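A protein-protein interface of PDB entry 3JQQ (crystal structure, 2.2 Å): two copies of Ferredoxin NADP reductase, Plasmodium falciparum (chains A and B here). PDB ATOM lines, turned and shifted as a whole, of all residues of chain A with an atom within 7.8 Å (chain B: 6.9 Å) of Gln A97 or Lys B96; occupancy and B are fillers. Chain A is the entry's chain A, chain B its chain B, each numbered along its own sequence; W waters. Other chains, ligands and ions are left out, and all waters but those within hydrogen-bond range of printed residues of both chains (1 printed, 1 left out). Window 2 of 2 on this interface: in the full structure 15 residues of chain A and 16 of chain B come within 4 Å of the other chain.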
ATOM      1  N   VAL A  12      20.776  19.874  27.993  1.00  0.00           N
ATOM      2  CA  VAL A  12      21.526  18.814  27.333  1.00  0.00           C
ATOM      3  C   VAL A  12      21.432  17.504  28.110  1.00  0.00           C
ATOM      4  O   VAL A  12      21.698  16.432  27.564  1.00  0.00           O
ATOM      5  CB  VAL A  12      23.006  19.192  27.110  1.00  0.00           C
ATOM      6  CG1 VAL A  12      23.130  20.209  25.983  1.00  0.00           C
ATOM      7  CG2 VAL A  12      23.622  19.723  28.395  1.00  0.00           C
ATOM      8  N   LYS A  13      21.040  17.591  29.379  1.00  0.00           N
ATOM      9  CA  LYS A  13      20.901  16.394  30.204  1.00  0.00           C
ATOM     10  C   LYS A  13      19.473  15.846  30.220  1.00  0.00           C
ATOM     11  O   LYS A  13      19.257  14.689  30.577  1.00  0.00           O
ATOM     12  CB  LYS A  13      21.421  16.629  31.627  1.00  0.00           C
ATOM     13  CG  LYS A  13      22.838  17.182  31.669  1.00  0.00           C
ATOM     14  CD  LYS A  13      23.761  16.315  32.512  1.00  0.00           C
ATOM     15  CE  LYS A  13      24.152  15.047  31.763  1.00  0.00           C
ATOM     16  NZ  LYS A  13      25.357  14.393  32.347  1.00  0.00           N
ATOM     17  N   ILE A  57      20.978  19.141  19.565  1.00  0.00           N
ATOM     18  CA  ILE A  57      22.156  18.359  19.908  1.00  0.00           C
ATOM     19  C   ILE A  57      22.411  17.349  18.801  1.00  0.00           C
ATOM     20  O   ILE A  57      21.691  16.357  18.686  1.00  0.00           O
ATOM     21  CB  ILE A  57      21.979  17.631  21.251  1.00  0.00           C
ATOM     22  CG1 ILE A  57      21.659  18.639  22.358  1.00  0.00           C
ATOM     23  CG2 ILE A  57      23.225  16.831  21.598  1.00  0.00           C
ATOM     24  CD1 ILE A  57      21.064  18.011  23.599  1.00  0.00           C
ATOM     25  N   PRO A  58      23.428  17.608  17.970  1.00  0.00           N
ATOM     26  CA  PRO A  58      23.695  16.755  16.819  1.00  0.00           C
ATOM     27  C   PRO A  58      24.054  15.329  17.222  1.00  0.00           C
ATOM     28  O   PRO A  58      24.837  15.124  18.148  1.00  0.00           O
ATOM     29  CB  PRO A  58      24.893  17.436  16.147  1.00  0.00           C
ATOM     30  CG  PRO A  58      24.839  18.851  16.614  1.00  0.00           C
ATOM     31  CD  PRO A  58      24.335  18.766  18.020  1.00  0.00           C
ATOM     32  N   TYR A  59      23.469  14.362  16.519  1.00  0.00           N
ATOM     33  CA  TYR A  59      23.758  12.943  16.715  1.00  0.00           C
ATOM     34  C   TYR A  59      23.482  12.458  18.135  1.00  0.00           C
ATOM     35  O   TYR A  59      24.070  11.472  18.583  1.00  0.00           O
ATOM     36  CB  TYR A  59      25.208  12.620  16.342  1.00  0.00           C
ATOM     37  CG  TYR A  59      25.657  13.139  14.993  1.00  0.00           C
ATOM     38  CD1 TYR A  59      26.451  14.276  14.898  1.00  0.00           C
ATOM     39  CD2 TYR A  59      25.303  12.486  13.818  1.00  0.00           C
ATOM     40  CE1 TYR A  59      26.874  14.753  13.673  1.00  0.00           C
ATOM     41  CE2 TYR A  59      25.722  12.958  12.588  1.00  0.00           C
ATOM     42  CZ  TYR A  59      26.507  14.091  12.522  1.00  0.00           C
ATOM     43  OH  TYR A  59      26.926  14.565  11.300  1.00  0.00           O
ATOM     44  N   TYR A  60      22.590  13.144  18.842  1.00  0.00           N
ATOM     45  CA  TYR A  60      22.260  12.747  20.205  1.00  0.00           C
ATOM     46  C   TYR A  60      21.658  11.345  20.249  1.00  0.00           C
ATOM     47  O   TYR A  60      20.749  11.018  19.482  1.00  0.00           O
ATOM     48  CB  TYR A  60      21.310  13.754  20.861  1.00  0.00           C
ATOM     49  CG  TYR A  60      21.034  13.470  22.325  1.00  0.00           C
ATOM     50  CD1 TYR A  60      21.920  13.883  23.313  1.00  0.00           C
ATOM     51  CD2 TYR A  60      19.888  12.789  22.716  1.00  0.00           C
ATOM     52  CE1 TYR A  60      21.671  13.624  24.651  1.00  0.00           C
ATOM     53  CE2 TYR A  60      19.632  12.526  24.051  1.00  0.00           C
ATOM     54  CZ  TYR A  60      20.525  12.945  25.013  1.00  0.00           C
ATOM     55  OH  TYR A  60      20.269  12.684  26.338  1.00  0.00           O
ATOM     56  N   ASN A  61      22.192  10.523  21.147  1.00  0.00           N
ATOM     57  CA  ASN A  61      21.609   9.226  21.478  1.00  0.00           C
ATOM     58  C   ASN A  61      20.789   8.602  20.351  1.00  0.00           C
ATOM     59  O   ASN A  61      21.301   7.789  19.579  1.00  0.00           O
ATOM     60  CB  ASN A  61      20.783   9.356  22.765  1.00  0.00           C
ATOM     61  CG  ASN A  61      19.535   8.501  22.755  1.00  0.00           C
ATOM     62  OD1 ASN A  61      19.539   7.374  22.255  1.00  0.00           O
ATOM     63  ND2 ASN A  61      18.453   9.032  23.318  1.00  0.00           N
ATOM     64  N   GLN A  97      29.125  13.764  21.399  1.00  0.00           N
ATOM     65  CA  GLN A  97      29.845  14.880  22.002  1.00  0.00           C
ATOM     66  C   GLN A  97      28.931  15.702  22.904  1.00  0.00           C
ATOM     67  O   GLN A  97      29.399  16.469  23.744  1.00  0.00           O
ATOM     68  CB  GLN A  97      30.455  15.770  20.919  1.00  0.00           C
ATOM     69  CG  GLN A  97      31.444  15.058  20.012  1.00  0.00           C
ATOM     70  CD  GLN A  97      32.028  15.972  18.954  1.00  0.00           C
ATOM     71  OE1 GLN A  97      31.695  17.155  18.886  1.00  0.00           O
ATOM     72  NE2 GLN A  97      32.904  15.425  18.118  1.00  0.00           N
ATOM     73  N   ARG A  98      27.624  15.535  22.725  1.00  0.00           N
ATOM     74  CA  ARG A  98      26.643  16.261  23.522  1.00  0.00           C
ATOM     75  C   ARG A  98      26.921  17.760  23.509  1.00  0.00           C
ATOM     76  O   ARG A  98      27.138  18.369  24.557  1.00  0.00           O
ATOM     77  CB  ARG A  98      26.630  15.740  24.961  1.00  0.00           C
ATOM     78  CG  ARG A  98      26.270  14.270  25.087  1.00  0.00           C
ATOM     79  CD  ARG A  98      26.279  13.820  26.538  1.00  0.00           C
ATOM     80  NE  ARG A  98      25.923  12.412  26.678  1.00  0.00           N
ATOM     81  CZ  ARG A  98      24.683  11.967  26.846  1.00  0.00           C
ATOM     82  NH1 ARG A  98      23.671  12.823  26.897  1.00  0.00           N
ATOM     83  NH2 ARG A  98      24.452  10.666  26.964  1.00  0.00           N
ATOM     84  N   CYS A  99      26.912  18.349  22.319  1.00  0.00           N
ATOM     85  CA  CYS A  99      27.162  19.773  22.168  1.00  0.00           C
ATOM     86  C   CYS A  99      25.987  20.369  21.426  1.00  0.00           C
ATOM     87  O   CYS A  99      25.617  19.885  20.357  1.00  0.00           O
ATOM     88  CB  CYS A  99      28.457  20.016  21.395  1.00  0.00           C
ATOM     89  SG  CYS A  99      29.933  19.321  22.173  1.00  0.00           S
ATOM     90  N   ALA A 100      25.388  21.412  21.985  1.00  0.00           N
ATOM     91  CA  ALA A 100      24.217  21.978  21.330  1.00  0.00           C
ATOM     92  C   ALA A 100      24.514  23.236  20.519  1.00  0.00           C
ATOM     93  O   ALA A 100      25.442  23.979  20.816  1.00  0.00           O
ATOM     94  CB  ALA A 100      23.113  22.248  22.343  1.00  0.00           C
ATOM     95  N   ARG A 101      23.711  23.454  19.482  1.00  0.00           N
ATOM     96  CA  ARG A 101      23.788  24.667  18.681  1.00  0.00           C
ATOM     97  C   ARG A 101      22.455  25.398  18.749  1.00  0.00           C
ATOM     98  O   ARG A 101      21.394  24.775  18.756  1.00  0.00           O
ATOM     99  CB  ARG A 101      24.117  24.335  17.225  1.00  0.00           C
ATOM    100  CG  ARG A 101      25.324  23.434  17.042  1.00  0.00           C
ATOM    101  CD  ARG A 101      26.622  24.197  17.234  1.00  0.00           C
ATOM    102  NE  ARG A 101      27.778  23.420  16.795  1.00  0.00           N
ATOM    103  CZ  ARG A 101      28.691  22.900  17.615  1.00  0.00           C
ATOM    104  NH1 ARG A 101      28.589  23.079  18.920  1.00  0.00           N
ATOM    105  NH2 ARG A 101      29.710  22.212  17.119  1.00  0.00           N
ATOM    106  N   TYR A 137      29.779  20.758  12.301  1.00  0.00           N
ATOM    107  CA  TYR A 137      29.303  19.605  13.075  1.00  0.00           C
ATOM    108  C   TYR A 137      27.791  19.442  12.960  1.00  0.00           C
ATOM    109  O   TYR A 137      27.308  18.416  12.482  1.00  0.00           O
ATOM    110  CB  TYR A 137      29.730  19.738  14.540  1.00  0.00           C
ATOM    111  CG  TYR A 137      29.367  18.567  15.432  1.00  0.00           C
ATOM    112  CD1 TYR A 137      29.911  17.306  15.225  1.00  0.00           C
ATOM    113  CD2 TYR A 137      28.501  18.734  16.504  1.00  0.00           C
ATOM    114  CE1 TYR A 137      29.589  16.242  16.050  1.00  0.00           C
ATOM    115  CE2 TYR A 137      28.176  17.679  17.334  1.00  0.00           C
ATOM    116  CZ  TYR A 137      28.721  16.437  17.104  1.00  0.00           C
ATOM    117  OH  TYR A 137      28.397  15.384  17.929  1.00  0.00           O
ATOM    118  N   VAL B  12      39.378  14.561  20.940  1.00  0.00           N
ATOM    119  CA  VAL B  12      38.474  14.804  22.047  1.00  0.00           C
ATOM    120  C   VAL B  12      38.495  13.598  22.979  1.00  0.00           C
ATOM    121  O   VAL B  12      38.131  13.698  24.151  1.00  0.00           O
ATOM    122  CB  VAL B  12      37.038  15.044  21.553  1.00  0.00           C
ATOM    123  CG1 VAL B  12      36.297  15.956  22.513  1.00  0.00           C
ATOM    124  CG2 VAL B  12      37.057  15.647  20.156  1.00  0.00           C
ATOM    125  N   ILE B  94      30.176  18.664  37.500  1.00  0.00           N
ATOM    126  CA  ILE B  94      30.001  19.142  36.132  1.00  0.00           C
ATOM    127  C   ILE B  94      29.354  18.087  35.235  1.00  0.00           C
ATOM    128  O   ILE B  94      28.939  17.027  35.706  1.00  0.00           O
ATOM    129  CB  ILE B  94      31.340  19.598  35.514  1.00  0.00           C
ATOM    130  CG1 ILE B  94      32.462  18.627  35.886  1.00  0.00           C
ATOM    131  CG2 ILE B  94      31.688  21.004  35.979  1.00  0.00           C
ATOM    132  CD1 ILE B  94      32.867  18.689  37.350  1.00  0.00           C
ATOM    133  N   LYS B  95      29.276  18.389  33.942  1.00  0.00           N
ATOM    134  CA  LYS B  95      28.642  17.503  32.968  1.00  0.00           C
ATOM    135  C   LYS B  95      29.658  16.999  31.940  1.00  0.00           C
ATOM    136  O   LYS B  95      30.833  17.361  31.995  1.00  0.00           O
ATOM    137  CB  LYS B  95      27.484  18.228  32.277  1.00  0.00           C
ATOM    138  CG  LYS B  95      26.443  18.772  33.248  1.00  0.00           C
ATOM    139  CD  LYS B  95      25.350  19.564  32.541  1.00  0.00           C
ATOM    140  CE  LYS B  95      25.824  20.955  32.149  1.00  0.00           C
ATOM    141  NZ  LYS B  95      24.701  21.802  31.657  1.00  0.00           N
ATOM    142  N   LYS B  96      29.207  16.165  31.008  1.00  0.00           N
ATOM    143  CA  LYS B  96      30.108  15.580  30.012  1.00  0.00           C
ATOM    144  C   LYS B  96      30.055  16.278  28.653  1.00  0.00           C
ATOM    145  O   LYS B  96      29.931  15.633  27.611  1.00  0.00           O
ATOM    146  CB  LYS B  96      29.863  14.075  29.871  1.00  0.00           C
ATOM    147  CG  LYS B  96      30.528  13.257  30.969  1.00  0.00           C
ATOM    148  CD  LYS B  96      29.983  11.841  31.047  1.00  0.00           C
ATOM    149  CE  LYS B  96      30.583  11.100  32.235  1.00  0.00           C
ATOM    150  NZ  LYS B  96      29.917   9.790  32.483  1.00  0.00           N
ATOM    151  N   GLN B  97      30.151  17.605  28.684  1.00  0.00           N
ATOM    152  CA  GLN B  97      30.253  18.413  27.475  1.00  0.00           C
ATOM    153  C   GLN B  97      31.695  18.465  26.986  1.00  0.00           C
ATOM    154  O   GLN B  97      32.486  19.268  27.480  1.00  0.00           O
ATOM    155  CB  GLN B  97      29.807  19.850  27.750  1.00  0.00           C
ATOM    156  CG  GLN B  97      28.313  20.095  27.752  1.00  0.00           C
ATOM    157  CD  GLN B  97      27.986  21.579  27.826  1.00  0.00           C
ATOM    158  OE1 GLN B  97      27.421  22.053  28.810  1.00  0.00           O
ATOM    159  NE2 GLN B  97      28.359  22.319  26.788  1.00  0.00           N
ATOM    160  N   ARG B  98      32.044  17.620  26.022  1.00  0.00           N
ATOM    161  CA  ARG B  98      33.338  17.752  25.361  1.00  0.00           C
ATOM    162  C   ARG B  98      33.166  18.510  24.051  1.00  0.00           C
ATOM    163  O   ARG B  98      33.049  17.911  22.984  1.00  0.00           O
ATOM    164  CB  ARG B  98      33.997  16.392  25.124  1.00  0.00           C
ATOM    165  CG  ARG B  98      34.675  15.817  26.361  1.00  0.00           C
ATOM    166  CD  ARG B  98      35.739  14.790  25.999  1.00  0.00           C
ATOM    167  NE  ARG B  98      35.219  13.738  25.131  1.00  0.00           N
ATOM    168  CZ  ARG B  98      35.768  12.532  25.011  1.00  0.00           C
ATOM    169  NH1 ARG B  98      36.853  12.222  25.710  1.00  0.00           N
ATOM    170  NH2 ARG B  98      35.228  11.634  24.196  1.00  0.00           N
ATOM    171  N   CYS B  99      33.155  19.835  24.152  1.00  0.00           N
ATOM    172  CA  CYS B  99      32.842  20.697  23.020  1.00  0.00           C
ATOM    173  C   CYS B  99      34.013  21.613  22.685  1.00  0.00           C
ATOM    174  O   CYS B  99      34.156  22.696  23.253  1.00  0.00           O
ATOM    175  CB  CYS B  99      31.592  21.511  23.339  1.00  0.00           C
ATOM    176  SG  CYS B  99      30.290  20.472  24.029  1.00  0.00           S
ATOM    177  N   ALA B 100      34.844  21.166  21.750  1.00  0.00           N
ATOM    178  CA  ALA B 100      36.107  21.830  21.448  1.00  0.00           C
ATOM    179  C   ALA B 100      35.969  22.957  20.431  1.00  0.00           C
ATOM    180  O   ALA B 100      35.142  22.896  19.525  1.00  0.00           O
ATOM    181  CB  ALA B 100      37.134  20.811  20.972  1.00  0.00           C
HETATM  182  O   HOH W   1      29.111  22.996  22.294  1.00  0.00           O
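SG of Cys A99 sits close to O of Arg B98, at 3.5 Å.
The side-chain sulfur (SG) of Cys A99 forms a disulfide with the side-chain sulfur (SG) of Cys B99.
Water W1 lies within hydrogen-bond range of the side-chain sulfur (SG) of Cys B99 (3.3 Å), the guanidinium group (NH1) of Arg A101 (3.4 Å) and the side-chain sulfur (SG) of Cys A99 (3.8 Å).
Gln A97 touches Arg B98, and with the chains exchanged Arg A98 touches Gln B97.
Arg A98 touches Cys B99, and with the chains exchanged Cys A99 touches Arg B98.
Cys B99 touches its own counterpart, Cys A99.
5 positions are printed for both chains.
O of Val B12 sits at hydrogen-bond distance from NH1 of Arg B98.
OH of Tyr A60 lies close to NH1 of Arg A98, at 3.5 Å.
Lys B95 touches Lys A13.
Gln A97 touches Lys B96.
O of Gln A97 touches N of Arg B98, at 3.7 Å.
Gln B97 touches Arg A98 (CG to O, 3.8 Å).
Arg A98 touches Cys B99.
Of the 8 printed residues of chain B, 5 touch a printed residue of chain A.
Printed residues of chain B that touch a printed residue of chain A: Lys B95, Lys B96, Gln B97, Arg B98 and Cys B99.
Along chain B the printed residues that touch a printed residue of chain A span positions 95 to 99.
Of the 13 printed residues of chain A, 4 touch a printed residue of chain B.
Along chain A the printed residues that touch a printed residue of chain B span positions 13 to 99.
Among the printed residues, 7 pairs touch across the chains.
Among the printed residues, no Asp or Glu carboxylate lies within 4 Å of a Lys or Arg side-chain nitrogen of the other chain.
Printed residues of chain B within 4 Å of Gln A97: Lys B96 and Arg B98.
Printed residues of chain A within 4 Å of Lys B96: Gln A97.
Of the printed residues of chain A, Gln B97 touches Arg A98 (3.8 Å).
Of the printed residues of chain B, Lys A13 touches Lys B95 (3.6 Å).
Printed residues of chain A within 4 Å of Lys B95: Lys A13 (3.6 Å).
Of the printed residues of chain B, Arg A98 touches Gln B97 and Cys B99.
Ala A100 touches none of the printed residues of chain B.
Asn A61 touches none of the printed residues of chain B.
The nearest printed residue of chain A that does not touch Lys B96 is Arg A98 (4.2 Å).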
